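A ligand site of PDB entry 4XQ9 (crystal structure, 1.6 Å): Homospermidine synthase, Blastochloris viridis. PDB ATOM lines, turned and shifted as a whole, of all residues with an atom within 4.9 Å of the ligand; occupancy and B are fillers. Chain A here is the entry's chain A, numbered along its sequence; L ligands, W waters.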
ATOM      1  N   ILE A  15      18.202  -3.452  10.994  1.00  0.00           N
ATOM      2  CA  ILE A  15      17.361  -2.461  10.342  1.00  0.00           C
ATOM      3  C   ILE A  15      17.993  -1.106  10.570  1.00  0.00           C
ATOM      4  O   ILE A  15      18.077  -0.620  11.703  1.00  0.00           O
ATOM      5  CB  ILE A  15      15.917  -2.479  10.861  1.00  0.00           C
ATOM      6  CG1 ILE A  15      15.331  -3.883  10.781  1.00  0.00           C
ATOM      7  CG2 ILE A  15      15.091  -1.500  10.054  1.00  0.00           C
ATOM      8  CD1 ILE A  15      13.944  -4.012  11.416  1.00  0.00           C
ATOM      9  N   GLY A  16      18.473  -0.518   9.488  1.00  0.00           N
ATOM     10  CA  GLY A  16      19.190   0.733   9.564  1.00  0.00           C
ATOM     11  C   GLY A  16      20.689   0.542   9.614  1.00  0.00           C
ATOM     12  O   GLY A  16      21.234  -0.247  10.409  1.00  0.00           O
ATOM     13  N   PHE A  17      21.370   1.326   8.785  1.00  0.00           N
ATOM     14  CA  PHE A  17      22.804   1.266   8.668  1.00  0.00           C
ATOM     15  C   PHE A  17      23.355   2.681   8.562  1.00  0.00           C
ATOM     16  O   PHE A  17      24.099   3.008   7.647  1.00  0.00           O
ATOM     17  CB  PHE A  17      23.203   0.415   7.466  1.00  0.00           C
ATOM     18  CG  PHE A  17      24.617  -0.115   7.533  1.00  0.00           C
ATOM     19  CD1 PHE A  17      25.035  -0.902   8.601  1.00  0.00           C
ATOM     20  CD2 PHE A  17      25.499   0.158   6.514  1.00  0.00           C
ATOM     21  CE1 PHE A  17      26.325  -1.376   8.656  1.00  0.00           C
ATOM     22  CE2 PHE A  17      26.798  -0.329   6.552  1.00  0.00           C
ATOM     23  CZ  PHE A  17      27.214  -1.096   7.633  1.00  0.00           C
ATOM     24  N   GLY A  18      22.921   3.517   9.502  1.00  0.00           N
ATOM     25  CA  GLY A  18      23.470   4.850   9.682  1.00  0.00           C
ATOM     26  C   GLY A  18      24.684   4.818  10.595  1.00  0.00           C
ATOM     27  O   GLY A  18      25.418   3.825  10.626  1.00  0.00           O
ATOM     28  N   SER A  19      24.888   5.887  11.366  1.00  0.00           N
ATOM     29  CA  SER A  19      26.076   5.940  12.205  1.00  0.00           C
ATOM     30  C   SER A  19      26.103   4.825  13.268  1.00  0.00           C
ATOM     31  O   SER A  19      27.160   4.229  13.522  1.00  0.00           O
ATOM     32  CB  SER A  19      26.223   7.341  12.842  1.00  0.00           C
ATOM     33  OG  SER A  19      25.493   7.488  14.051  1.00  0.00           O
ATOM     34  N   ILE A  20      24.968   4.500  13.865  1.00  0.00           N
ATOM     35  CA  ILE A  20      24.969   3.477  14.915  1.00  0.00           C
ATOM     36  C   ILE A  20      25.055   2.070  14.285  1.00  0.00           C
ATOM     37  O   ILE A  20      25.781   1.217  14.777  1.00  0.00           O
ATOM     38  CB  ILE A  20      23.729   3.598  15.813  1.00  0.00           C
ATOM     39  CG1 ILE A  20      23.678   5.004  16.455  1.00  0.00           C
ATOM     40  CG2 ILE A  20      23.740   2.519  16.895  1.00  0.00           C
ATOM     41  CD1 ILE A  20      24.988   5.484  17.063  1.00  0.00           C
ATOM     42  N   GLY A  21      24.340   1.823  13.188  1.00  0.00           N
ATOM     43  CA  GLY A  21      24.459   0.560  12.495  1.00  0.00           C
ATOM     44  C   GLY A  21      25.881   0.248  12.066  1.00  0.00           C
ATOM     45  O   GLY A  21      26.375  -0.872  12.224  1.00  0.00           O
ATOM     46  N   ARG A  22      26.569   1.254  11.528  1.00  0.00           N
ATOM     47  CA  ARG A  22      27.920   1.060  11.043  1.00  0.00           C
ATOM     48  C   ARG A  22      28.882   0.752  12.191  1.00  0.00           C
ATOM     49  O   ARG A  22      29.860   0.058  11.989  1.00  0.00           O
ATOM     50  CB  ARG A  22      28.381   2.299  10.275  1.00  0.00           C
ATOM     51  CG  ARG A  22      27.627   2.453   8.964  1.00  0.00           C
ATOM     52  CD  ARG A  22      27.781   3.853   8.354  1.00  0.00           C
ATOM     53  NE  ARG A  22      26.629   4.134   7.510  1.00  0.00           N
ATOM     54  CZ  ARG A  22      26.501   5.179   6.705  1.00  0.00           C
ATOM     55  NH1 ARG A  22      27.465   6.085   6.583  1.00  0.00           N
ATOM     56  NH2 ARG A  22      25.373   5.306   6.015  1.00  0.00           N
ATOM     57  N   ILE A  42      19.185  -3.950   6.251  1.00  0.00           N
ATOM     58  CA  ILE A  42      18.118  -3.305   5.499  1.00  0.00           C
ATOM     59  C   ILE A  42      18.166  -1.790   5.707  1.00  0.00           C
ATOM     60  O   ILE A  42      18.074  -1.321   6.844  1.00  0.00           O
ATOM     61  CB  ILE A  42      16.718  -3.803   5.940  1.00  0.00           C
ATOM     62  CG1 ILE A  42      16.649  -5.337   5.909  1.00  0.00           C
ATOM     63  CG2 ILE A  42      15.624  -3.205   5.066  1.00  0.00           C
ATOM     64  CD1 ILE A  42      15.406  -5.852   6.562  1.00  0.00           C
ATOM     65  N   ASP A  43      18.303  -1.039   4.612  1.00  0.00           N
ATOM     66  CA  ASP A  43      18.383   0.423   4.670  1.00  0.00           C
ATOM     67  C   ASP A  43      18.105   1.003   3.266  1.00  0.00           C
ATOM     68  O   ASP A  43      18.638   0.500   2.290  1.00  0.00           O
ATOM     69  CB  ASP A  43      19.760   0.849   5.183  1.00  0.00           C
ATOM     70  CG  ASP A  43      19.833   2.309   5.583  1.00  0.00           C
ATOM     71  OD1 ASP A  43      19.452   3.192   4.768  1.00  0.00           O
ATOM     72  OD2 ASP A  43      20.292   2.582   6.708  1.00  0.00           O
ATOM     73  N   PRO A  44      17.282   2.056   3.168  1.00  0.00           N
ATOM     74  CA  PRO A  44      16.950   2.597   1.830  1.00  0.00           C
ATOM     75  C   PRO A  44      18.062   3.400   1.163  1.00  0.00           C
ATOM     76  O   PRO A  44      18.017   3.656  -0.053  1.00  0.00           O
ATOM     77  CB  PRO A  44      15.740   3.498   2.120  1.00  0.00           C
ATOM     78  CG  PRO A  44      15.935   3.919   3.569  1.00  0.00           C
ATOM     79  CD  PRO A  44      16.458   2.675   4.221  1.00  0.00           C
ATOM     80  N   SER A  45      19.066   3.787   1.937  1.00  0.00           N
ATOM     81  CA  SER A  45      20.099   4.713   1.490  1.00  0.00           C
ATOM     82  C   SER A  45      21.143   4.095   0.547  1.00  0.00           C
ATOM     83  O   SER A  45      21.671   3.006   0.801  1.00  0.00           O
ATOM     84  CB  SER A  45      20.792   5.325   2.718  1.00  0.00           C
ATOM     85  OG  SER A  45      22.132   5.658   2.454  1.00  0.00           O
ATOM     86  N   ALA A  48      24.489   3.968   2.352  1.00  0.00           N
ATOM     87  CA  ALA A  48      24.562   2.789   3.195  1.00  0.00           C
ATOM     88  C   ALA A  48      24.845   1.525   2.368  1.00  0.00           C
ATOM     89  O   ALA A  48      25.634   0.688   2.791  1.00  0.00           O
ATOM     90  CB  ALA A  48      23.276   2.635   3.992  1.00  0.00           C
ATOM     91  N   GLN A  62      15.873  -1.083   1.013  1.00  0.00           N
ATOM     92  CA  GLN A  62      14.443  -0.875   1.118  1.00  0.00           C
ATOM     93  C   GLN A  62      14.117  -0.168   2.427  1.00  0.00           C
ATOM     94  O   GLN A  62      14.670  -0.496   3.467  1.00  0.00           O
ATOM     95  CB  GLN A  62      13.683  -2.213   1.041  1.00  0.00           C
ATOM     96  CG  GLN A  62      12.180  -2.098   0.848  1.00  0.00           C
ATOM     97  CD  GLN A  62      11.795  -1.719  -0.570  1.00  0.00           C
ATOM     98  OE1 GLN A  62      12.495  -2.060  -1.526  1.00  0.00           O
ATOM     99  NE2 GLN A  62      10.708  -0.986  -0.715  1.00  0.00           N
ATOM    100  N   ALA A  63      13.228   0.811   2.344  1.00  0.00           N
ATOM    101  CA  ALA A  63      12.591   1.384   3.526  1.00  0.00           C
ATOM    102  C   ALA A  63      11.560   0.431   4.101  1.00  0.00           C
ATOM    103  O   ALA A  63      10.690  -0.074   3.394  1.00  0.00           O
ATOM    104  CB  ALA A  63      11.934   2.731   3.173  1.00  0.00           C
ATOM    105  N   VAL A  64      11.669   0.170   5.395  1.00  0.00           N
ATOM    106  CA  VAL A  64      10.666  -0.569   6.136  1.00  0.00           C
ATOM    107  C   VAL A  64       9.510   0.376   6.454  1.00  0.00           C
ATOM    108  O   VAL A  64       9.708   1.427   7.073  1.00  0.00           O
ATOM    109  CB  VAL A  64      11.229  -1.170   7.437  1.00  0.00           C
ATOM    110  CG1 VAL A  64      10.154  -1.879   8.230  1.00  0.00           C
ATOM    111  CG2 VAL A  64      12.378  -2.122   7.121  1.00  0.00           C
ATOM    112  N   LEU A  89      18.106  -0.241  14.368  1.00  0.00           N
ATOM    113  CA  LEU A  89      18.925   0.958  14.530  1.00  0.00           C
ATOM    114  C   LEU A  89      18.535   1.980  13.482  1.00  0.00           C
ATOM    115  O   LEU A  89      19.395   2.615  12.871  1.00  0.00           O
ATOM    116  CB  LEU A  89      20.406   0.600  14.417  1.00  0.00           C
ATOM    117  CG  LEU A  89      20.884  -0.472  15.400  1.00  0.00           C
ATOM    118  CD1 LEU A  89      22.318  -0.865  15.097  1.00  0.00           C
ATOM    119  CD2 LEU A  89      20.763   0.017  16.838  1.00  0.00           C
ATOM    120  N   SER A  90      17.236   2.137  13.267  1.00  0.00           N
ATOM    121  CA  SER A  90      16.722   2.985  12.196  1.00  0.00           C
ATOM    122  C   SER A  90      16.029   4.238  12.698  1.00  0.00           C
ATOM    123  O   SER A  90      15.854   4.443  13.909  1.00  0.00           O
ATOM    124  CB  SER A  90      15.758   2.174  11.334  1.00  0.00           C
ATOM    125  OG  SER A  90      14.662   1.697  12.126  1.00  0.00           O
ATOM    126  N   VAL A  91      15.635   5.089  11.757  1.00  0.00           N
ATOM    127  CA  VAL A  91      14.670   6.152  11.993  1.00  0.00           C
ATOM    128  C   VAL A  91      13.426   5.865  11.144  1.00  0.00           C
ATOM    129  O   VAL A  91      13.489   5.067  10.204  1.00  0.00           O
ATOM    130  CB  VAL A  91      15.222   7.546  11.628  1.00  0.00           C
ATOM    131  CG1 VAL A  91      16.383   7.919  12.540  1.00  0.00           C
ATOM    132  CG2 VAL A  91      15.634   7.616  10.140  1.00  0.00           C
ATOM    133  N   ASP A  92      12.303   6.506  11.490  1.00  0.00           N
ATOM    134  CA  ASP A  92      11.072   6.474  10.675  1.00  0.00           C
ATOM    135  C   ASP A  92      10.348   5.117  10.681  1.00  0.00           C
ATOM    136  O   ASP A  92       9.418   4.911   9.894  1.00  0.00           O
ATOM    137  CB  ASP A  92      11.358   6.871   9.212  1.00  0.00           C
ATOM    138  CG  ASP A  92      11.885   8.311   9.075  1.00  0.00           C
ATOM    139  OD1 ASP A  92      11.759   9.102  10.028  1.00  0.00           O
ATOM    140  OD2 ASP A  92      12.409   8.641   7.984  1.00  0.00           O
ATOM    141  N   THR A  93      10.743   4.236  11.580  1.00  0.00           N
ATOM    142  CA  THR A  93      10.101   2.933  11.718  1.00  0.00           C
ATOM    143  C   THR A  93       9.528   2.812  13.115  1.00  0.00           C
ATOM    144  O   THR A  93      10.054   3.386  14.066  1.00  0.00           O
ATOM    145  CB  THR A  93      11.085   1.787  11.459  1.00  0.00           C
ATOM    146  OG1 THR A  93      12.120   1.796  12.449  1.00  0.00           O
ATOM    147  CG2 THR A  93      11.728   1.910  10.052  1.00  0.00           C
ATOM    148  N   THR A 112      17.171   1.329  20.283  1.00  0.00           N
ATOM    149  CA  THR A 112      17.802   2.362  21.088  1.00  0.00           C
ATOM    150  C   THR A 112      16.899   3.559  21.308  1.00  0.00           C
ATOM    151  O   THR A 112      17.354   4.576  21.795  1.00  0.00           O
ATOM    152  CB  THR A 112      19.103   2.857  20.454  1.00  0.00           C
ATOM    153  OG1 THR A 112      18.817   3.570  19.245  1.00  0.00           O
ATOM    154  CG2 THR A 112      20.025   1.684  20.151  1.00  0.00           C
ATOM    155  N   VAL A 113      15.639   3.429  20.902  1.00  0.00           N
ATOM    156  CA  VAL A 113      14.672   4.522  20.935  1.00  0.00           C
ATOM    157  C   VAL A 113      13.269   3.940  20.682  1.00  0.00           C
ATOM    158  O   VAL A 113      13.141   2.920  20.011  1.00  0.00           O
ATOM    159  CB  VAL A 113      14.996   5.571  19.861  1.00  0.00           C
ATOM    160  CG1 VAL A 113      15.000   4.916  18.482  1.00  0.00           C
ATOM    161  CG2 VAL A 113      14.016   6.754  19.914  1.00  0.00           C
ATOM    162  N   GLU A 115      10.735   4.687  18.495  1.00  0.00           N
ATOM    163  CA  GLU A 115      10.502   5.462  17.286  1.00  0.00           C
ATOM    164  C   GLU A 115       9.096   5.157  16.760  1.00  0.00           C
ATOM    165  O   GLU A 115       8.635   4.019  16.883  1.00  0.00           O
ATOM    166  CB  GLU A 115      11.564   5.115  16.233  1.00  0.00           C
ATOM    167  CG  GLU A 115      11.534   5.922  14.931  1.00  0.00           C
ATOM    168  CD  GLU A 115      12.172   7.302  15.043  1.00  0.00           C
ATOM    169  OE1 GLU A 115      12.516   7.711  16.168  1.00  0.00           O
ATOM    170  OE2 GLU A 115      12.321   7.970  13.988  1.00  0.00           O
ATOM    171  N   GLY A 158      20.570   1.970  24.109  1.00  0.00           N
ATOM    172  CA  GLY A 158      21.762   2.634  23.581  1.00  0.00           C
ATOM    173  C   GLY A 158      22.607   3.184  24.718  1.00  0.00           C
ATOM    174  O   GLY A 158      22.659   2.592  25.802  1.00  0.00           O
ATOM    175  N   ALA A 159      23.260   4.316  24.484  1.00  0.00           N
ATOM    176  CA  ALA A 159      24.034   4.984  25.524  1.00  0.00           C
ATOM    177  C   ALA A 159      23.104   5.713  26.481  1.00  0.00           C
ATOM    178  O   ALA A 159      23.247   5.602  27.688  1.00  0.00           O
ATOM    179  CB  ALA A 159      25.037   5.948  24.901  1.00  0.00           C
ATOM    180  N   ASN A 160      22.165   6.458  25.919  1.00  0.00           N
ATOM    181  CA  ASN A 160      21.190   7.234  26.687  1.00  0.00           C
ATOM    182  C   ASN A 160      20.008   7.548  25.777  1.00  0.00           C
ATOM    183  O   ASN A 160      20.124   8.414  24.916  1.00  0.00           O
ATOM    184  CB  ASN A 160      21.805   8.520  27.281  1.00  0.00           C
ATOM    185  CG  ASN A 160      22.500   9.419  26.249  1.00  0.00           C
ATOM    186  OD1 ASN A 160      23.185   8.977  25.329  1.00  0.00           O
ATOM    187  ND2 ASN A 160      22.335  10.718  26.437  1.00  0.00           N
ATOM    188  N   PRO A 161      18.876   6.833  25.953  1.00  0.00           N
ATOM    189  CA  PRO A 161      18.621   5.811  26.965  1.00  0.00           C
ATOM    190  C   PRO A 161      19.450   4.543  26.791  1.00  0.00           C
ATOM    191  O   PRO A 161      19.893   4.237  25.687  1.00  0.00           O
ATOM    192  CB  PRO A 161      17.132   5.489  26.774  1.00  0.00           C
ATOM    193  CG  PRO A 161      16.878   5.796  25.343  1.00  0.00           C
ATOM    194  CD  PRO A 161      17.702   7.025  25.077  1.00  0.00           C
ATOM    195  N   TRP A 227      26.090  12.188  15.643  1.00  0.00           N
ATOM    196  CA  TRP A 227      25.167  11.069  15.471  1.00  0.00           C
ATOM    197  C   TRP A 227      23.971  11.608  14.680  1.00  0.00           C
ATOM    198  O   TRP A 227      24.006  12.754  14.279  1.00  0.00           O
ATOM    199  CB  TRP A 227      24.751  10.476  16.833  1.00  0.00           C
ATOM    200  CG  TRP A 227      24.034  11.431  17.754  1.00  0.00           C
ATOM    201  CD1 TRP A 227      24.590  12.426  18.529  1.00  0.00           C
ATOM    202  CD2 TRP A 227      22.637  11.453  18.025  1.00  0.00           C
ATOM    203  NE1 TRP A 227      23.593  13.086  19.233  1.00  0.00           N
ATOM    204  CE2 TRP A 227      22.390  12.490  18.948  1.00  0.00           C
ATOM    205  CE3 TRP A 227      21.550  10.697  17.555  1.00  0.00           C
ATOM    206  CZ2 TRP A 227      21.104  12.785  19.407  1.00  0.00           C
ATOM    207  CZ3 TRP A 227      20.278  10.993  18.015  1.00  0.00           C
ATOM    208  CH2 TRP A 227      20.066  12.026  18.940  1.00  0.00           C
ATOM    209  N   SER A 228      22.945  10.784  14.461  1.00  0.00           N
ATOM    210  CA  SER A 228      21.788  11.154  13.616  1.00  0.00           C
ATOM    211  C   SER A 228      21.399  12.628  13.703  1.00  0.00           C
ATOM    212  O   SER A 228      21.052  13.103  14.778  1.00  0.00           O
ATOM    213  CB  SER A 228      20.571  10.327  14.013  1.00  0.00           C
ATOM    214  OG  SER A 228      19.550  10.436  13.033  1.00  0.00           O
ATOM    215  N   VAL A 229      21.440  13.335  12.589  1.00  0.00           N
ATOM    216  CA  VAL A 229      20.868  14.685  12.557  1.00  0.00           C
ATOM    217  C   VAL A 229      19.342  14.608  12.563  1.00  0.00           C
ATOM    218  O   VAL A 229      18.675  15.330  13.316  1.00  0.00           O
ATOM    219  CB  VAL A 229      21.364  15.462  11.332  1.00  0.00           C
ATOM    220  CG1 VAL A 229      20.589  16.772  11.161  1.00  0.00           C
ATOM    221  CG2 VAL A 229      22.872  15.718  11.462  1.00  0.00           C
ATOM    222  N   GLY A 231      17.436  12.223  13.701  1.00  0.00           N
ATOM    223  CA  GLY A 231      17.016  11.802  15.021  1.00  0.00           C
ATOM    224  C   GLY A 231      17.141  12.891  16.082  1.00  0.00           C
ATOM    225  O   GLY A 231      16.269  13.034  16.937  1.00  0.00           O
ATOM    226  N   TRP A 346      22.730  18.403   5.774  1.00  0.00           N
ATOM    227  CA  TRP A 346      23.288  17.989   7.070  1.00  0.00           C
ATOM    228  C   TRP A 346      24.386  16.958   6.878  1.00  0.00           C
ATOM    229  O   TRP A 346      24.467  16.320   5.836  1.00  0.00           O
ATOM    230  CB  TRP A 346      22.212  17.409   7.986  1.00  0.00           C
ATOM    231  CG  TRP A 346      21.442  16.221   7.459  1.00  0.00           C
ATOM    232  CD1 TRP A 346      20.206  16.256   6.864  1.00  0.00           C
ATOM    233  CD2 TRP A 346      21.825  14.826   7.503  1.00  0.00           C
ATOM    234  NE1 TRP A 346      19.810  14.981   6.527  1.00  0.00           N
ATOM    235  CE2 TRP A 346      20.780  14.088   6.911  1.00  0.00           C
ATOM    236  CE3 TRP A 346      22.945  14.137   7.985  1.00  0.00           C
ATOM    237  CZ2 TRP A 346      20.823  12.696   6.776  1.00  0.00           C
ATOM    238  CZ3 TRP A 346      22.981  12.751   7.848  1.00  0.00           C
ATOM    239  CH2 TRP A 346      21.926  12.049   7.253  1.00  0.00           C
ATOM    240  N   ILE A 348      26.926  14.060   9.371  1.00  0.00           N
ATOM    241  CA  ILE A 348      27.395  13.473  10.622  1.00  0.00           C
ATOM    242  C   ILE A 348      28.914  13.315  10.575  1.00  0.00           C
ATOM    243  O   ILE A 348      29.477  12.788   9.609  1.00  0.00           O
ATOM    244  CB  ILE A 348      26.728  12.106  10.878  1.00  0.00           C
ATOM    245  CG1 ILE A 348      25.223  12.282  11.014  1.00  0.00           C
ATOM    246  CG2 ILE A 348      27.287  11.451  12.135  1.00  0.00           C
ATOM    247  CD1 ILE A 348      24.438  10.996  10.896  1.00  0.00           C
ATOM    248  N   VAL A 398      27.177   4.061  22.105  1.00  0.00           N
ATOM    249  CA  VAL A 398      25.871   3.528  21.762  1.00  0.00           C
ATOM    250  C   VAL A 398      25.994   2.092  21.272  1.00  0.00           C
ATOM    251  O   VAL A 398      25.263   1.205  21.712  1.00  0.00           O
ATOM    252  CB  VAL A 398      25.180   4.381  20.674  1.00  0.00           C
ATOM    253  CG1 VAL A 398      23.785   3.783  20.353  1.00  0.00           C
ATOM    254  CG2 VAL A 398      25.104   5.849  21.100  1.00  0.00           C
HETATM  255  P1  LIG L   1      21.339   7.943  11.168  1.00  0.00           P
HETATM  256  O1  LIG L   1      20.551   9.119  10.823  1.00  0.00           O
HETATM  257  O2  LIG L   1      22.720   8.063  11.015  1.00  0.00           O
HETATM  258  O3  LIG L   1      20.899   6.675  10.326  1.00  0.00           O
HETATM  259  C1  LIG L   1      19.577   6.284  10.228  1.00  0.00           C
HETATM  260  C2  LIG L   1      19.387   5.215   9.169  1.00  0.00           C
HETATM  261  O4  LIG L   1      18.053   4.800   9.091  1.00  0.00           O
HETATM  262  C3  LIG L   1      19.769   5.796   7.801  1.00  0.00           C
HETATM  263  O5  LIG L   1      20.863   5.152   7.124  1.00  0.00           O
HETATM  264  C4  LIG L   1      18.480   5.765   7.037  1.00  0.00           C
HETATM  265  O6  LIG L   1      18.614   5.539   5.652  1.00  0.00           O
HETATM  266  C5  LIG L   1      17.705   4.676   7.754  1.00  0.00           C
HETATM  267  N1  LIG L   1      16.269   4.646   7.487  1.00  0.00           N
HETATM  268  C6  LIG L   1      15.414   5.629   7.265  1.00  0.00           C
HETATM  269  N2  LIG L   1      14.217   5.168   7.057  1.00  0.00           N
HETATM  270  C7  LIG L   1      14.283   3.874   7.143  1.00  0.00           C
HETATM  271  C8  LIG L   1      13.343   2.795   6.999  1.00  0.00           C
HETATM  272  N3  LIG L   1      12.085   3.094   6.732  1.00  0.00           N
HETATM  273  N4  LIG L   1      13.779   1.582   7.137  1.00  0.00           N
HETATM  274  C9  LIG L   1      15.015   1.314   7.391  1.00  0.00           C
HETATM  275  N5  LIG L   1      15.928   2.245   7.526  1.00  0.00           N
HETATM  276  C10 LIG L   1      15.629   3.520   7.410  1.00  0.00           C
HETATM  277  O7  LIG L   1      21.003   7.548  12.661  1.00  0.00           O
HETATM  278  P2  LIG L   1      21.909   6.892  13.756  1.00  0.00           P
HETATM  279  O8  LIG L   1      22.424   5.650  13.256  1.00  0.00           O
HETATM  280  O9  LIG L   1      22.871   7.837  14.270  1.00  0.00           O
HETATM  281  O10 LIG L   1      20.895   6.579  14.873  1.00  0.00           O
HETATM  282  C11 LIG L   1      19.947   5.627  14.585  1.00  0.00           C
HETATM  283  C12 LIG L   1      18.879   5.504  15.652  1.00  0.00           C
HETATM  284  O11 LIG L   1      19.421   5.342  16.897  1.00  0.00           O
HETATM  285  C13 LIG L   1      18.036   6.765  15.690  1.00  0.00           C
HETATM  286  O12 LIG L   1      16.700   6.370  15.743  1.00  0.00           O
HETATM  287  C14 LIG L   1      18.515   7.518  16.905  1.00  0.00           C
HETATM  288  O13 LIG L   1      17.625   8.288  17.603  1.00  0.00           O
HETATM  289  C15 LIG L   1      18.942   6.341  17.776  1.00  0.00           C
HETATM  290  N6  LIG L   1      19.994   6.654  18.749  1.00  0.00           N
HETATM  291  C16 LIG L   1      19.882   6.296  20.020  1.00  0.00           C
HETATM  292  C17 LIG L   1      20.857   6.586  20.926  1.00  0.00           C
HETATM  293  C18 LIG L   1      20.838   6.220  22.384  1.00  0.00           C
HETATM  294  O14 LIG L   1      21.807   6.492  22.976  1.00  0.00           O
HETATM  295  N7  LIG L   1      19.859   5.557  22.959  1.00  0.00           N
HETATM  296  C19 LIG L   1      21.965   7.216  20.483  1.00  0.00           C
HETATM  297  C20 LIG L   1      22.087   7.532  19.196  1.00  0.00           C
HETATM  298  C21 LIG L   1      21.099   7.227  18.338  1.00  0.00           C
HETATM  299  O   HOH W   1      22.884   6.611   6.405  1.00  0.00           O
HETATM  300  O   HOH W   2      14.826   8.961  16.322  1.00  0.00           O
HETATM  301  O   HOH W   3      22.007   3.216  12.141  1.00  0.00           O
HETATM  302  O   HOH W   4      12.170   6.986   5.967  1.00  0.00           O
HETATM  303  O   HOH W   5      10.093   5.272   5.361  1.00  0.00           O
HETATM  304  O   HOH W   6      17.998   7.571   4.045  1.00  0.00           O
HETATM  305  O   HOH W   7      15.451   8.930   6.952  1.00  0.00           O
HETATM  306  O   HOH W   8      18.851   9.192   8.433  1.00  0.00           O
HETATM  307  O   HOH W   9      20.920   9.831  22.756  1.00  0.00           O
HETATM  308  O   HOH W  10      20.578  11.889  10.140  1.00  0.00           O
HETATM  309  O   HOH W  11      24.219   8.082   8.535  1.00  0.00           O
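The backbone NH (N) of Ala 48 sits at hydrogen-bond distance from the side-chain hydroxyl (OG) of Ser 45 (2.9 Å). The backbone NH of Gln 62 is in hydrogen-bond range of the backbone carbonyl oxygen of Asp 43, at 3.4 Å. The side-chain carboxylate (OD2) of Asp 43 is in hydrogen-bond range of the backbone NH (N) of Phe 17 (2.7 Å). The side-chain hydroxyl of Ser 228 lies within hydrogen-bond range of the backbone NH of Gly 231, 2.8 Å away. OG1 of Thr 93 is in hydrogen-bond range of OG of Ser 90, 2.6 Å away. N of Asp 92 is in hydrogen-bond range of OE2 of Glu 115, at 2.9 Å. OD1 of Asp 43 sits at hydrogen-bond distance from N of Ser 45 (2.9 Å). NE of Arg 22 sits close to O of Gly 18, 3.4 Å away.
Water W1 bridges an oxygen (O5) of the ligand and the guanidinium group of Arg 22. Water W3 lies within hydrogen-bond range of O8 of the ligand (2.7 Å), O of Leu 89 (2.8 Å), N of Gly 18 (2.8 Å) and N of Gly 21 (2.9 Å). Water W10 lies within hydrogen-bond range of an oxygen (O1) of the ligand, the backbone NH (N) of Val 229 and the side-chain hydroxyl (OG) of Ser 228. Water W4 lies within hydrogen-bond range of the side-chain carboxylate of Asp 92 (2.6 Å) and a nitrogen (N2) of the ligand (2.9 Å). Water W2 lies within hydrogen-bond range of OE1 of Glu 115 (2.6 Å) and O13 of the ligand (3.2 Å). Water W9 lies within hydrogen-bond range of the backbone carbonyl oxygen (O) of Asn 160 (2.7 Å) and an oxygen (O14) of the ligand (3.5 Å).
O of Val 91 lies close to N2 of the ligand, at 3.2 Å. Ile 15 touches the ligand (CG2 to C9, 3.9 Å). Phe 17 touches the ligand. Gly 18 touches the ligand (CA to O3, 3.2 Å). Pro 44 touches the ligand. CB of Ser 45 touches O6 of the ligand, at 3.7 Å. CB of Ala 63 touches N3 of the ligand, at 3.6 Å. Leu 89 touches the ligand. Asp 92 touches the ligand. Thr 93 touches the ligand (CG2 to N3, 3.5 Å). Val 113 touches the ligand (CG1 to O12, 3.5 Å). Gly 158 touches the ligand. Trp 227 touches the ligand (CE3 to C21, 3.6 Å). Ile 348 touches the ligand. Val 398 touches the ligand (CG2 to C19, 3.5 Å). Hydrophobic or aromatic side chains within 4 Å of the ligand: Ile 15, Ile 20, Pro 44, Ala 63, Val 64, Val 91, Val 113, Ala 159, Pro 161, Trp 227, Ile 348 and Val 398. The nearest printed residue that does not touch the ligand is Ile 42 (4.1 Å).
OG of Ser 228 lies within hydrogen-bond range of O1 of the ligand, at 2.8 Å. The backbone carbonyl oxygen (O) of Ser 90 lies within hydrogen-bond range of an oxygen (O12) of the ligand (2.8 Å). O of Val 64 sits at hydrogen-bond distance from N3 of the ligand (2.9 Å). O8 of the ligand is in hydrogen-bond range of N of Ile 20 (2.9 Å). An oxygen (O14) of the ligand is in hydrogen-bond range of the backbone NH (N) of Asn 160 (3.0 Å). O of Asn 160 sits close to N7 of the ligand. O of Thr 112 is in hydrogen-bond range of N7 of the ligand (2.9 Å). The side-chain hydroxyl (OG1) of Thr 112 sits at hydrogen-bond distance from an oxygen (O11) of the ligand, 3.0 Å away. O of Pro 161 is in hydrogen-bond range of N7 of the ligand (3.0 Å). The side-chain carboxylate (OD1) of Asp 43 lies within hydrogen-bond range of an oxygen (O6) of the ligand (2.6 Å). N of Ser 19 lies within hydrogen-bond range of O2 of the ligand, at 3.1 Å. N of Ala 159 is in hydrogen-bond range of O14 of the ligand, 3.0 Å away. The backbone NH of Val 64 sits at hydrogen-bond distance from a nitrogen (N4) of the ligand (3.1 Å). N of Ser 228 lies within hydrogen-bond range of O9 of the ligand (3.0 Å). OG of Ser 19 is in hydrogen-bond range of O9 of the ligand (2.7 Å).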
